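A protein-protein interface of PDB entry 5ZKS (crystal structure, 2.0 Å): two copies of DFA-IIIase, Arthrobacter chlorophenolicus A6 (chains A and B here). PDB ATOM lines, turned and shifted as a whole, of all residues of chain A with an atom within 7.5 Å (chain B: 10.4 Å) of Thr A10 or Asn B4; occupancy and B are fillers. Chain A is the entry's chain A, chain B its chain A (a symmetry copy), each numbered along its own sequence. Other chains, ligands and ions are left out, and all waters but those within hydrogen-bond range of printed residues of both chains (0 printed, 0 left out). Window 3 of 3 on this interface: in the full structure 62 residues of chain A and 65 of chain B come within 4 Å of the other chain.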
ATOM      1  N   TYR A   7     -17.810 -23.075   0.127  1.00  0.00           N
ATOM      2  CA  TYR A   7     -18.062 -24.228   0.983  1.00  0.00           C
ATOM      3  C   TYR A   7     -17.165 -24.228   2.208  1.00  0.00           C
ATOM      4  O   TYR A   7     -15.997 -23.855   2.143  1.00  0.00           O
ATOM      5  CB  TYR A   7     -17.771 -25.521   0.250  1.00  0.00           C
ATOM      6  CG  TYR A   7     -18.528 -25.768  -1.022  1.00  0.00           C
ATOM      7  CD1 TYR A   7     -18.123 -25.174  -2.220  1.00  0.00           C
ATOM      8  CD2 TYR A   7     -19.600 -26.662  -1.056  1.00  0.00           C
ATOM      9  CE1 TYR A   7     -18.791 -25.423  -3.403  1.00  0.00           C
ATOM     10  CE2 TYR A   7     -20.265 -26.923  -2.246  1.00  0.00           C
ATOM     11  CZ  TYR A   7     -19.854 -26.301  -3.407  1.00  0.00           C
ATOM     12  OH  TYR A   7     -20.505 -26.547  -4.586  1.00  0.00           O
ATOM     13  N   ASP A   8     -17.704 -24.712   3.310  1.00  0.00           N
ATOM     14  CA  ASP A   8     -16.949 -24.835   4.550  1.00  0.00           C
ATOM     15  C   ASP A   8     -16.999 -26.316   4.851  1.00  0.00           C
ATOM     16  O   ASP A   8     -18.091 -26.884   4.946  1.00  0.00           O
ATOM     17  CB  ASP A   8     -17.623 -24.002   5.649  1.00  0.00           C
ATOM     18  CG  ASP A   8     -16.993 -24.185   7.013  1.00  0.00           C
ATOM     19  OD1 ASP A   8     -16.591 -25.317   7.360  1.00  0.00           O
ATOM     20  OD2 ASP A   8     -16.928 -23.194   7.765  1.00  0.00           O
ATOM     21  N   VAL A   9     -15.838 -26.946   4.996  1.00  0.00           N
ATOM     22  CA  VAL A   9     -15.801 -28.405   5.135  1.00  0.00           C
ATOM     23  C   VAL A   9     -16.465 -28.912   6.399  1.00  0.00           C
ATOM     24  O   VAL A   9     -16.835 -30.085   6.450  1.00  0.00           O
ATOM     25  CB  VAL A   9     -14.387 -28.984   5.096  1.00  0.00           C
ATOM     26  CG1 VAL A   9     -13.705 -28.584   3.797  1.00  0.00           C
ATOM     27  CG2 VAL A   9     -13.584 -28.569   6.333  1.00  0.00           C
ATOM     28  N   THR A  10     -16.596 -28.054   7.413  1.00  0.00           N
ATOM     29  CA  THR A  10     -17.352 -28.422   8.636  1.00  0.00           C
ATOM     30  C   THR A  10     -18.874 -28.285   8.471  1.00  0.00           C
ATOM     31  O   THR A  10     -19.635 -28.692   9.337  1.00  0.00           O
ATOM     32  CB  THR A  10     -16.892 -27.626   9.886  1.00  0.00           C
ATOM     33  OG1 THR A  10     -17.228 -26.243   9.753  1.00  0.00           O
ATOM     34  CG2 THR A  10     -15.389 -27.749  10.091  1.00  0.00           C
ATOM     35  N   GLU A  11     -19.321 -27.701   7.368  1.00  0.00           N
ATOM     36  CA  GLU A  11     -20.739 -27.524   7.122  1.00  0.00           C
ATOM     37  C   GLU A  11     -21.224 -28.364   5.930  1.00  0.00           C
ATOM     38  O   GLU A  11     -22.340 -28.180   5.479  1.00  0.00           O
ATOM     39  CB  GLU A  11     -21.050 -26.035   6.941  1.00  0.00           C
ATOM     40  CG  GLU A  11     -20.701 -25.219   8.188  1.00  0.00           C
ATOM     41  CD  GLU A  11     -21.053 -23.746   8.092  1.00  0.00           C
ATOM     42  OE1 GLU A  11     -21.207 -23.235   6.962  1.00  0.00           O
ATOM     43  OE2 GLU A  11     -21.161 -23.096   9.161  1.00  0.00           O
ATOM     44  N   TRP A  12     -20.408 -29.294   5.437  1.00  0.00           N
ATOM     45  CA  TRP A  12     -20.810 -30.128   4.293  1.00  0.00           C
ATOM     46  C   TRP A  12     -21.502 -31.388   4.824  1.00  0.00           C
ATOM     47  O   TRP A  12     -20.965 -32.052   5.708  1.00  0.00           O
ATOM     48  CB  TRP A  12     -19.612 -30.495   3.399  1.00  0.00           C
ATOM     49  CG  TRP A  12     -20.017 -31.136   2.091  1.00  0.00           C
ATOM     50  CD1 TRP A  12     -19.709 -32.400   1.662  1.00  0.00           C
ATOM     51  CD2 TRP A  12     -20.826 -30.549   1.058  1.00  0.00           C
ATOM     52  NE1 TRP A  12     -20.271 -32.628   0.423  1.00  0.00           N
ATOM     53  CE2 TRP A  12     -20.968 -31.514   0.036  1.00  0.00           C
ATOM     54  CE3 TRP A  12     -21.450 -29.308   0.905  1.00  0.00           C
ATOM     55  CZ2 TRP A  12     -21.697 -31.271  -1.121  1.00  0.00           C
ATOM     56  CZ3 TRP A  12     -22.182 -29.065  -0.246  1.00  0.00           C
ATOM     57  CH2 TRP A  12     -22.296 -30.042  -1.248  1.00  0.00           C
ATOM     58  N   PRO A  13     -22.695 -31.722   4.293  1.00  0.00           N
ATOM     59  CA  PRO A  13     -23.476 -32.841   4.875  1.00  0.00           C
ATOM     60  C   PRO A  13     -22.999 -34.279   4.615  1.00  0.00           C
ATOM     61  O   PRO A  13     -23.580 -35.201   5.187  1.00  0.00           O
ATOM     62  CB  PRO A  13     -24.882 -32.665   4.281  1.00  0.00           C
ATOM     63  CG  PRO A  13     -24.869 -31.442   3.458  1.00  0.00           C
ATOM     64  CD  PRO A  13     -23.475 -30.920   3.332  1.00  0.00           C
ATOM     65  N   PRO A  17     -15.126 -34.408   8.286  1.00  0.00           N
ATOM     66  CA  PRO A  17     -13.789 -33.924   7.958  1.00  0.00           C
ATOM     67  C   PRO A  17     -12.711 -34.294   8.971  1.00  0.00           C
ATOM     68  O   PRO A  17     -11.544 -34.332   8.602  1.00  0.00           O
ATOM     69  CB  PRO A  17     -13.978 -32.404   7.891  1.00  0.00           C
ATOM     70  CG  PRO A  17     -15.114 -32.140   8.831  1.00  0.00           C
ATOM     71  CD  PRO A  17     -16.045 -33.292   8.583  1.00  0.00           C
ATOM     72  N   ALA A  18     -13.082 -34.542  10.228  1.00  0.00           N
ATOM     73  CA  ALA A  18     -12.125 -35.012  11.232  1.00  0.00           C
ATOM     74  C   ALA A  18     -11.576 -36.388  10.846  1.00  0.00           C
ATOM     75  O   ALA A  18     -10.384 -36.647  11.025  1.00  0.00           O
ATOM     76  CB  ALA A  18     -12.767 -35.073  12.616  1.00  0.00           C
ATOM     77  N   ILE A  21     -11.236 -35.925   5.605  1.00  0.00           N
ATOM     78  CA  ILE A  21     -11.460 -34.671   4.890  1.00  0.00           C
ATOM     79  C   ILE A  21     -11.317 -34.855   3.369  1.00  0.00           C
ATOM     80  O   ILE A  21     -11.905 -34.106   2.558  1.00  0.00           O
ATOM     81  CB  ILE A  21     -10.508 -33.558   5.440  1.00  0.00           C
ATOM     82  CG1 ILE A  21     -10.842 -32.169   4.899  1.00  0.00           C
ATOM     83  CG2 ILE A  21      -9.050 -33.834   5.106  1.00  0.00           C
ATOM     84  CD1 ILE A  21     -12.309 -31.909   4.726  1.00  0.00           C
ATOM     85  N   VAL A  24     -14.684 -35.610   1.985  1.00  0.00           N
ATOM     86  CA  VAL A  24     -15.517 -34.402   2.044  1.00  0.00           C
ATOM     87  C   VAL A  24     -15.215 -33.450   0.892  1.00  0.00           C
ATOM     88  O   VAL A  24     -16.122 -32.960   0.222  1.00  0.00           O
ATOM     89  CB  VAL A  24     -15.323 -33.658   3.385  1.00  0.00           C
ATOM     90  CG1 VAL A  24     -16.053 -32.325   3.378  1.00  0.00           C
ATOM     91  CG2 VAL A  24     -15.823 -34.510   4.547  1.00  0.00           C
ATOM     92  N   ILE A  28     -17.442 -32.240  -2.327  1.00  0.00           N
ATOM     93  CA  ILE A  28     -17.664 -30.851  -2.686  1.00  0.00           C
ATOM     94  C   ILE A  28     -17.308 -30.605  -4.154  1.00  0.00           C
ATOM     95  O   ILE A  28     -18.044 -29.895  -4.870  1.00  0.00           O
ATOM     96  CB  ILE A  28     -16.867 -29.896  -1.763  1.00  0.00           C
ATOM     97  CG1 ILE A  28     -17.490 -29.883  -0.364  1.00  0.00           C
ATOM     98  CG2 ILE A  28     -16.858 -28.482  -2.335  1.00  0.00           C
ATOM     99  CD1 ILE A  28     -16.554 -29.405   0.736  1.00  0.00           C
ATOM    100  N   TYR A  52     -13.290 -23.766   2.320  1.00  0.00           N
ATOM    101  CA  TYR A  52     -12.678 -23.178   3.508  1.00  0.00           C
ATOM    102  C   TYR A  52     -12.511 -24.236   4.588  1.00  0.00           C
ATOM    103  O   TYR A  52     -13.447 -24.978   4.892  1.00  0.00           O
ATOM    104  CB  TYR A  52     -13.510 -21.997   4.045  1.00  0.00           C
ATOM    105  CG  TYR A  52     -13.018 -21.467   5.393  1.00  0.00           C
ATOM    106  CD1 TYR A  52     -11.756 -20.888   5.511  1.00  0.00           C
ATOM    107  CD2 TYR A  52     -13.808 -21.549   6.540  1.00  0.00           C
ATOM    108  CE1 TYR A  52     -11.286 -20.416   6.725  1.00  0.00           C
ATOM    109  CE2 TYR A  52     -13.345 -21.078   7.762  1.00  0.00           C
ATOM    110  CZ  TYR A  52     -12.080 -20.508   7.846  1.00  0.00           C
ATOM    111  OH  TYR A  52     -11.599 -20.031   9.051  1.00  0.00           O
ATOM    112  N   LEU A  53     -11.308 -24.303   5.147  1.00  0.00           N
ATOM    113  CA  LEU A  53     -11.008 -25.161   6.289  1.00  0.00           C
ATOM    114  C   LEU A  53     -10.747 -24.279   7.506  1.00  0.00           C
ATOM    115  O   LEU A  53      -9.705 -23.643   7.585  1.00  0.00           O
ATOM    116  CB  LEU A  53      -9.759 -25.990   6.024  1.00  0.00           C
ATOM    117  CG  LEU A  53      -9.819 -27.143   5.020  1.00  0.00           C
ATOM    118  CD1 LEU A  53     -10.249 -26.641   3.660  1.00  0.00           C
ATOM    119  CD2 LEU A  53      -8.455 -27.796   4.932  1.00  0.00           C
ATOM    120  N   PRO A  54     -11.684 -24.261   8.467  1.00  0.00           N
ATOM    121  CA  PRO A  54     -11.441 -23.594   9.732  1.00  0.00           C
ATOM    122  C   PRO A  54     -10.317 -24.295  10.478  1.00  0.00           C
ATOM    123  O   PRO A  54      -9.979 -25.439  10.139  1.00  0.00           O
ATOM    124  CB  PRO A  54     -12.771 -23.746  10.502  1.00  0.00           C
ATOM    125  CG  PRO A  54     -13.753 -24.356   9.566  1.00  0.00           C
ATOM    126  CD  PRO A  54     -13.004 -24.922   8.405  1.00  0.00           C
ATOM    127  N   PRO A  55      -9.721 -23.622  11.476  1.00  0.00           N
ATOM    128  CA  PRO A  55      -8.681 -24.291  12.256  1.00  0.00           C
ATOM    129  C   PRO A  55      -9.222 -25.578  12.884  1.00  0.00           C
ATOM    130  O   PRO A  55     -10.348 -25.604  13.386  1.00  0.00           O
ATOM    131  CB  PRO A  55      -8.293 -23.232  13.288  1.00  0.00           C
ATOM    132  CG  PRO A  55      -8.593 -21.934  12.592  1.00  0.00           C
ATOM    133  CD  PRO A  55      -9.867 -22.206  11.850  1.00  0.00           C
ATOM    134  N   GLY A  56      -8.441 -26.648  12.807  1.00  0.00           N
ATOM    135  CA  GLY A  56      -8.941 -27.979  13.156  1.00  0.00           C
ATOM    136  C   GLY A  56      -7.932 -29.045  12.787  1.00  0.00           C
ATOM    137  O   GLY A  56      -6.998 -28.791  12.034  1.00  0.00           O
ATOM    138  N   TYR A  58      -7.674 -32.393  10.846  1.00  0.00           N
ATOM    139  CA  TYR A  58      -8.482 -33.114   9.856  1.00  0.00           C
ATOM    140  C   TYR A  58      -7.687 -34.227   9.254  1.00  0.00           C
ATOM    141  O   TYR A  58      -6.702 -33.969   8.586  1.00  0.00           O
ATOM    142  CB  TYR A  58      -8.910 -32.196   8.718  1.00  0.00           C
ATOM    143  CG  TYR A  58      -9.630 -30.964   9.166  1.00  0.00           C
ATOM    144  CD1 TYR A  58     -10.924 -31.032   9.662  1.00  0.00           C
ATOM    145  CD2 TYR A  58      -9.017 -29.717   9.078  1.00  0.00           C
ATOM    146  CE1 TYR A  58     -11.602 -29.879  10.065  1.00  0.00           C
ATOM    147  CE2 TYR A  58      -9.671 -28.571   9.469  1.00  0.00           C
ATOM    148  CZ  TYR A  58     -10.965 -28.654   9.966  1.00  0.00           C
ATOM    149  OH  TYR A  58     -11.610 -27.517  10.372  1.00  0.00           O
ATOM    150  N   ASN B   4     -16.003 -24.712  13.239  1.00  0.00           N
ATOM    151  CA  ASN B   4     -15.708 -23.847  14.419  1.00  0.00           C
ATOM    152  C   ASN B   4     -14.187 -23.790  14.729  1.00  0.00           C
ATOM    153  O   ASN B   4     -13.379 -24.192  13.881  1.00  0.00           O
ATOM    154  CB  ASN B   4     -16.607 -24.218  15.627  1.00  0.00           C
ATOM    155  CG  ASN B   4     -15.988 -25.247  16.575  1.00  0.00           C
ATOM    156  OD1 ASN B   4     -15.402 -26.249  16.154  1.00  0.00           O
ATOM    157  ND2 ASN B   4     -16.150 -25.008  17.880  1.00  0.00           N
ATOM    158  N   ASN B   5     -13.829 -23.289  15.924  1.00  0.00           N
ATOM    159  CA  ASN B   5     -12.545 -22.638  16.196  1.00  0.00           C
ATOM    160  C   ASN B   5     -12.470 -21.342  15.403  1.00  0.00           C
ATOM    161  O   ASN B   5     -11.397 -20.831  15.189  1.00  0.00           O
ATOM    162  CB  ASN B   5     -11.331 -23.509  15.863  1.00  0.00           C
ATOM    163  CG  ASN B   5     -11.228 -24.746  16.731  1.00  0.00           C
ATOM    164  OD1 ASN B   5     -11.412 -24.694  17.956  1.00  0.00           O
ATOM    165  ND2 ASN B   5     -10.929 -25.866  16.107  1.00  0.00           N
ATOM    166  N   ARG B   6     -13.603 -20.827  14.940  1.00  0.00           N
ATOM    167  CA  ARG B   6     -13.622 -19.535  14.249  1.00  0.00           C
ATOM    168  C   ARG B   6     -14.496 -18.618  15.079  1.00  0.00           C
ATOM    169  O   ARG B   6     -15.624 -18.969  15.426  1.00  0.00           O
ATOM    170  CB  ARG B   6     -14.155 -19.645  12.810  1.00  0.00           C
ATOM    171  CG  ARG B   6     -14.012 -18.334  12.015  1.00  0.00           C
ATOM    172  CD  ARG B   6     -14.529 -18.411  10.577  1.00  0.00           C
ATOM    173  NE  ARG B   6     -15.921 -18.870  10.557  1.00  0.00           N
ATOM    174  CZ  ARG B   6     -16.706 -18.925   9.483  1.00  0.00           C
ATOM    175  NH1 ARG B   6     -16.271 -18.537   8.287  1.00  0.00           N
ATOM    176  NH2 ARG B   6     -17.955 -19.370   9.617  1.00  0.00           N
ATOM    177  N   TYR B   7     -13.966 -17.459  15.433  1.00  0.00           N
ATOM    178  CA  TYR B   7     -14.712 -16.492  16.228  1.00  0.00           C
ATOM    179  C   TYR B   7     -14.749 -15.126  15.566  1.00  0.00           C
ATOM    180  O   TYR B   7     -13.777 -14.683  14.961  1.00  0.00           O
ATOM    181  CB  TYR B   7     -14.062 -16.285  17.580  1.00  0.00           C
ATOM    182  CG  TYR B   7     -13.890 -17.499  18.446  1.00  0.00           C
ATOM    183  CD1 TYR B   7     -12.826 -18.379  18.237  1.00  0.00           C
ATOM    184  CD2 TYR B   7     -14.737 -17.730  19.532  1.00  0.00           C
ATOM    185  CE1 TYR B   7     -12.639 -19.480  19.051  1.00  0.00           C
ATOM    186  CE2 TYR B   7     -14.544 -18.829  20.358  1.00  0.00           C
ATOM    187  CZ  TYR B   7     -13.497 -19.692  20.108  1.00  0.00           C
ATOM    188  OH  TYR B   7     -13.298 -20.782  20.914  1.00  0.00           O
ATOM    189  N   ASP B   8     -15.858 -14.435  15.745  1.00  0.00           N
ATOM    190  CA  ASP B   8     -16.020 -13.084  15.223  1.00  0.00           C
ATOM    191  C   ASP B   8     -16.274 -12.254  16.462  1.00  0.00           C
ATOM    192  O   ASP B   8     -17.208 -12.547  17.213  1.00  0.00           O
ATOM    193  CB  ASP B   8     -17.207 -13.044  14.251  1.00  0.00           C
ATOM    194  CG  ASP B   8     -17.544 -11.648  13.771  1.00  0.00           C
ATOM    195  OD1 ASP B   8     -17.461 -10.687  14.566  1.00  0.00           O
ATOM    196  OD2 ASP B   8     -17.930 -11.512  12.594  1.00  0.00           O
ATOM    197  N   TRP B  12     -19.395 -12.440  19.788  1.00  0.00           N
ATOM    198  CA  TRP B  12     -19.032 -13.110  21.046  1.00  0.00           C
ATOM    199  C   TRP B  12     -19.931 -12.571  22.165  1.00  0.00           C
ATOM    200  O   TRP B  12     -20.059 -11.358  22.313  1.00  0.00           O
ATOM    201  CB  TRP B  12     -17.546 -12.916  21.395  1.00  0.00           C
ATOM    202  CG  TRP B  12     -17.082 -13.787  22.540  1.00  0.00           C
ATOM    203  CD1 TRP B  12     -16.603 -13.369  23.754  1.00  0.00           C
ATOM    204  CD2 TRP B  12     -17.080 -15.224  22.583  1.00  0.00           C
ATOM    205  NE1 TRP B  12     -16.297 -14.460  24.542  1.00  0.00           N
ATOM    206  CE2 TRP B  12     -16.589 -15.607  23.852  1.00  0.00           C
ATOM    207  CE3 TRP B  12     -17.455 -16.221  21.677  1.00  0.00           C
ATOM    208  CZ2 TRP B  12     -16.455 -16.936  24.229  1.00  0.00           C
ATOM    209  CZ3 TRP B  12     -17.327 -17.548  22.053  1.00  0.00           C
ATOM    210  CH2 TRP B  12     -16.827 -17.895  23.318  1.00  0.00           C
ATOM    211  N   ILE B  28     -12.370 -15.000  24.464  1.00  0.00           N
ATOM    212  CA  ILE B  28     -12.297 -15.982  23.398  1.00  0.00           C
ATOM    213  C   ILE B  28     -11.115 -16.930  23.610  1.00  0.00           C
ATOM    214  O   ILE B  28     -11.247 -18.155  23.410  1.00  0.00           O
ATOM    215  CB  ILE B  28     -12.210 -15.301  22.009  1.00  0.00           C
ATOM    216  CG1 ILE B  28     -13.556 -14.665  21.655  1.00  0.00           C
ATOM    217  CG2 ILE B  28     -11.823 -16.317  20.938  1.00  0.00           C
ATOM    218  CD1 ILE B  28     -13.476 -13.572  20.596  1.00  0.00           C
ATOM    219  N   ASP B  31     -11.899 -19.519  26.131  1.00  0.00           N
ATOM    220  CA  ASP B  31     -12.778 -20.533  25.534  1.00  0.00           C
ATOM    221  C   ASP B  31     -12.006 -21.566  24.697  1.00  0.00           C
ATOM    222  O   ASP B  31     -12.288 -22.781  24.730  1.00  0.00           O
ATOM    223  CB  ASP B  31     -13.851 -19.882  24.649  1.00  0.00           C
ATOM    224  CG  ASP B  31     -14.831 -20.899  24.101  1.00  0.00           C
ATOM    225  OD1 ASP B  31     -15.642 -21.372  24.911  1.00  0.00           O
ATOM    226  OD2 ASP B  31     -14.777 -21.243  22.889  1.00  0.00           O
ATOM    227  N   ILE B  32     -11.014 -21.093  23.956  1.00  0.00           N
ATOM    228  CA  ILE B  32     -10.181 -21.996  23.117  1.00  0.00           C
ATOM    229  C   ILE B  32      -9.444 -22.969  24.044  1.00  0.00           C
ATOM    230  O   ILE B  32      -9.456 -24.124  23.769  1.00  0.00           O
ATOM    231  CB  ILE B  32      -9.203 -21.198  22.237  1.00  0.00           C
ATOM    232  CG1 ILE B  32      -9.924 -20.358  21.187  1.00  0.00           C
ATOM    233  CG2 ILE B  32      -8.166 -22.101  21.618  1.00  0.00           C
ATOM    234  CD1 ILE B  32      -9.119 -19.214  20.691  1.00  0.00           C
ATOM    235  N   ALA B  34     -10.186 -23.843  27.117  1.00  0.00           N
ATOM    236  CA  ALA B  34     -11.153 -24.718  27.801  1.00  0.00           C
ATOM    237  C   ALA B  34     -11.529 -25.878  26.885  1.00  0.00           C
ATOM    238  O   ALA B  34     -11.661 -26.951  27.377  1.00  0.00           O
ATOM    239  CB  ALA B  34     -12.355 -23.929  28.198  1.00  0.00           C
ATOM    240  N   ARG B  35     -11.659 -25.618  25.593  1.00  0.00           N
ATOM    241  CA  ARG B  35     -12.055 -26.658  24.621  1.00  0.00           C
ATOM    242  C   ARG B  35     -10.846 -27.506  24.222  1.00  0.00           C
ATOM    243  O   ARG B  35     -10.998 -28.690  24.102  1.00  0.00           O
ATOM    244  CB  ARG B  35     -12.688 -25.998  23.403  1.00  0.00           C
ATOM    245  CG  ARG B  35     -14.015 -25.336  23.708  1.00  0.00           C
ATOM    246  CD  ARG B  35     -14.730 -24.924  22.452  1.00  0.00           C
ATOM    247  NE  ARG B  35     -14.015 -23.937  21.686  1.00  0.00           N
ATOM    248  CZ  ARG B  35     -13.250 -24.201  20.653  1.00  0.00           C
ATOM    249  NH1 ARG B  35     -12.432 -23.287  20.194  1.00  0.00           N
ATOM    250  NH2 ARG B  35     -13.310 -25.376  20.078  1.00  0.00           N
ATOM    251  N   GLN B  36      -9.686 -26.889  24.082  1.00  0.00           N
ATOM    252  CA  GLN B  36      -8.464 -27.583  23.620  1.00  0.00           C
ATOM    253  C   GLN B  36      -7.565 -27.928  24.809  1.00  0.00           C
ATOM    254  O   GLN B  36      -6.477 -27.422  24.883  1.00  0.00           O
ATOM    255  CB  GLN B  36      -7.798 -26.742  22.535  1.00  0.00           C
ATOM    256  CG  GLN B  36      -8.750 -26.368  21.415  1.00  0.00           C
ATOM    257  CD  GLN B  36      -8.122 -25.642  20.255  1.00  0.00           C
ATOM    258  OE1 GLN B  36      -6.931 -25.461  20.194  1.00  0.00           O
ATOM    259  NE2 GLN B  36      -8.942 -25.248  19.310  1.00  0.00           N
ATOM    260  N   PRO B  47      -5.298 -27.402  17.896  1.00  0.00           N
ATOM    261  CA  PRO B  47      -5.044 -26.781  16.596  1.00  0.00           C
ATOM    262  C   PRO B  47      -5.080 -25.258  16.591  1.00  0.00           C
ATOM    263  O   PRO B  47      -4.680 -24.656  15.590  1.00  0.00           O
ATOM    264  CB  PRO B  47      -6.184 -27.314  15.729  1.00  0.00           C
ATOM    265  CG  PRO B  47      -7.288 -27.543  16.694  1.00  0.00           C
ATOM    266  CD  PRO B  47      -6.601 -28.089  17.916  1.00  0.00           C
ATOM    267  N   GLY B  48      -5.563 -24.653  17.675  1.00  0.00           N
ATOM    268  CA  GLY B  48      -5.683 -23.212  17.760  1.00  0.00           C
ATOM    269  C   GLY B  48      -6.980 -22.695  17.167  1.00  0.00           C
ATOM    270  O   GLY B  48      -8.004 -23.390  17.159  1.00  0.00           O
ATOM    271  N   ALA B  49      -6.933 -21.449  16.697  1.00  0.00           N
ATOM    272  CA  ALA B  49      -8.129 -20.738  16.308  1.00  0.00           C
ATOM    273  C   ALA B  49      -7.863 -19.472  15.483  1.00  0.00           C
ATOM    274  O   ALA B  49      -6.715 -19.034  15.309  1.00  0.00           O
ATOM    275  CB  ALA B  49      -8.958 -20.411  17.550  1.00  0.00           C
ATOM    276  N   VAL B  50      -8.950 -18.935  14.933  1.00  0.00           N
ATOM    277  CA  VAL B  50      -8.946 -17.684  14.171  1.00  0.00           C
ATOM    278  C   VAL B  50      -9.994 -16.768  14.799  1.00  0.00           C
ATOM    279  O   VAL B  50     -11.124 -17.181  15.130  1.00  0.00           O
ATOM    280  CB  VAL B  50      -9.152 -17.896  12.638  1.00  0.00           C
ATOM    281  CG1 VAL B  50     -10.470 -18.583  12.339  1.00  0.00           C
ATOM    282  CG2 VAL B  50      -9.077 -16.579  11.863  1.00  0.00           C
ATOM    283  N   ILE B  51      -9.572 -15.536  15.041  1.00  0.00           N
ATOM    284  CA  ILE B  51     -10.414 -14.499  15.620  1.00  0.00           C
ATOM    285  C   ILE B  51     -10.517 -13.385  14.576  1.00  0.00           C
ATOM    286  O   ILE B  51      -9.504 -12.831  14.150  1.00  0.00           O
ATOM    287  CB  ILE B  51      -9.813 -13.966  16.937  1.00  0.00           C
ATOM    288  CG1 ILE B  51      -9.685 -15.093  17.966  1.00  0.00           C
ATOM    289  CG2 ILE B  51     -10.681 -12.852  17.496  1.00  0.00           C
ATOM    290  CD1 ILE B  51      -8.879 -14.726  19.190  1.00  0.00           C
ATOM    291  N   PHE B  70      -0.655 -21.295  17.297  1.00  0.00           N
ATOM    292  CA  PHE B  70      -1.558 -21.372  16.137  1.00  0.00           C
ATOM    293  C   PHE B  70      -2.798 -20.493  16.311  1.00  0.00           C
ATOM    294  O   PHE B  70      -3.894 -20.828  15.866  1.00  0.00           O
ATOM    295  CB  PHE B  70      -1.955 -22.815  15.838  1.00  0.00           C
ATOM    296  CG  PHE B  70      -0.895 -23.819  16.171  1.00  0.00           C
ATOM    297  CD1 PHE B  70       0.353 -23.751  15.586  1.00  0.00           C
ATOM    298  CD2 PHE B  70      -1.149 -24.825  17.084  1.00  0.00           C
ATOM    299  CE1 PHE B  70       1.331 -24.681  15.894  1.00  0.00           C
ATOM    300  CE2 PHE B  70      -0.179 -25.765  17.389  1.00  0.00           C
ATOM    301  CZ  PHE B  70       1.064 -25.688  16.799  1.00  0.00           C
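No residue of chain B comes within 4 Å of Asp A8.
Of the printed residues of chain B, Thr A10 touches Asn B4 (3.9996 Å).
No residue of chain B comes within 4 Å of Glu A11.
Of the printed residues of chain B, Tyr A52 touches Arg B6 (3.7 Å) and Val B50 (3.8 Å).
Printed residues of chain B within 4 Å of Pro A55: Asn B4, Asn B5, Gly B48, Ala B49 and Val B50.
Of the printed residues of chain B, Gly A56 touches Pro B47 (3.8 Å).
Printed residues of chain A within 4 Å of Asn B4: Thr A10 (3.9996 Å), Pro A54 (3.5 Å) and Pro A55 (3.4 Å).
Of the printed residues of chain A, Arg B6 touches Tyr A52 (3.7 Å).
Ile B28 touches none of the printed residues of chain A.
Of the printed residues of chain A, Val B50 touches Tyr A52 (3.8 Å) and Pro A55 (3.7 Å).
The nearest printed residue of chain B that does not touch Thr A10 is Arg B6 (6.9 Å).
The nearest printed residue of chain A that does not touch Asn B4 is Tyr A58 (5.1 Å).
ND2 of Asn B5 lies within hydrogen-bond range of O of Pro A55 (2.8 Å).
The backbone carbonyl oxygen (O) of Pro A55 lies close to the backbone carbonyl oxygen (O) of Asn B4 (3.4 Å).
Positions printed for both chains: 7, 8, 12 and 28.
Asn B4 touches Thr A10 (N to OG1, 3.9996 Å).
OH of Tyr A52 touches CD of Arg B6, 3.7 Å away.
Tyr A52 touches Val B50.
Asn B4 touches Pro A54.
Gly B48 touches Pro A55.
Pro A55 touches Ala B49 (CG to C, 3.9 Å).
CD of Pro A55 touches CG1 of Val B50, 3.7 Å away.
Pro B47 touches Gly A56.
Of the 18 printed residues of chain A, 5 touch a printed residue of chain B.
Of the 18 printed residues of chain B, 7 touch a printed residue of chain A.
Printed residues of chain B that touch a printed residue of chain A: Asn B4, Asn B5, Arg B6, Pro B47, Gly B48, Ala B49 and Val B50.
Hydrophobic or aromatic side chains of chain B within 4 Å of the printed part of chain A: Pro B47 and Val B50.
Among the printed residues, 10 pairs touch across the chains.
The backbone NH (N) of Val A9 is in hydrogen-bond range of the backbone carbonyl oxygen (O) of Tyr A52 (3.1 Å).
The backbone carbonyl oxygen (O) of Pro A54 sits at hydrogen-bond distance from the side-chain hydroxyl (OH) of Tyr A58, 2.7 Å away.
The backbone carbonyl oxygen of Asn B5 is in hydrogen-bond range of the backbone NH of Val B50.
The backbone NH of Tyr B7 sits at hydrogen-bond distance from the backbone carbonyl oxygen of Val B50, 2.9 Å away.
N of Gly B48 sits at hydrogen-bond distance from OE1 of Gln B36 (3.0 Å).
O of Phe B70 lies within hydrogen-bond range of N of Ala B49, at 3.2 Å.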
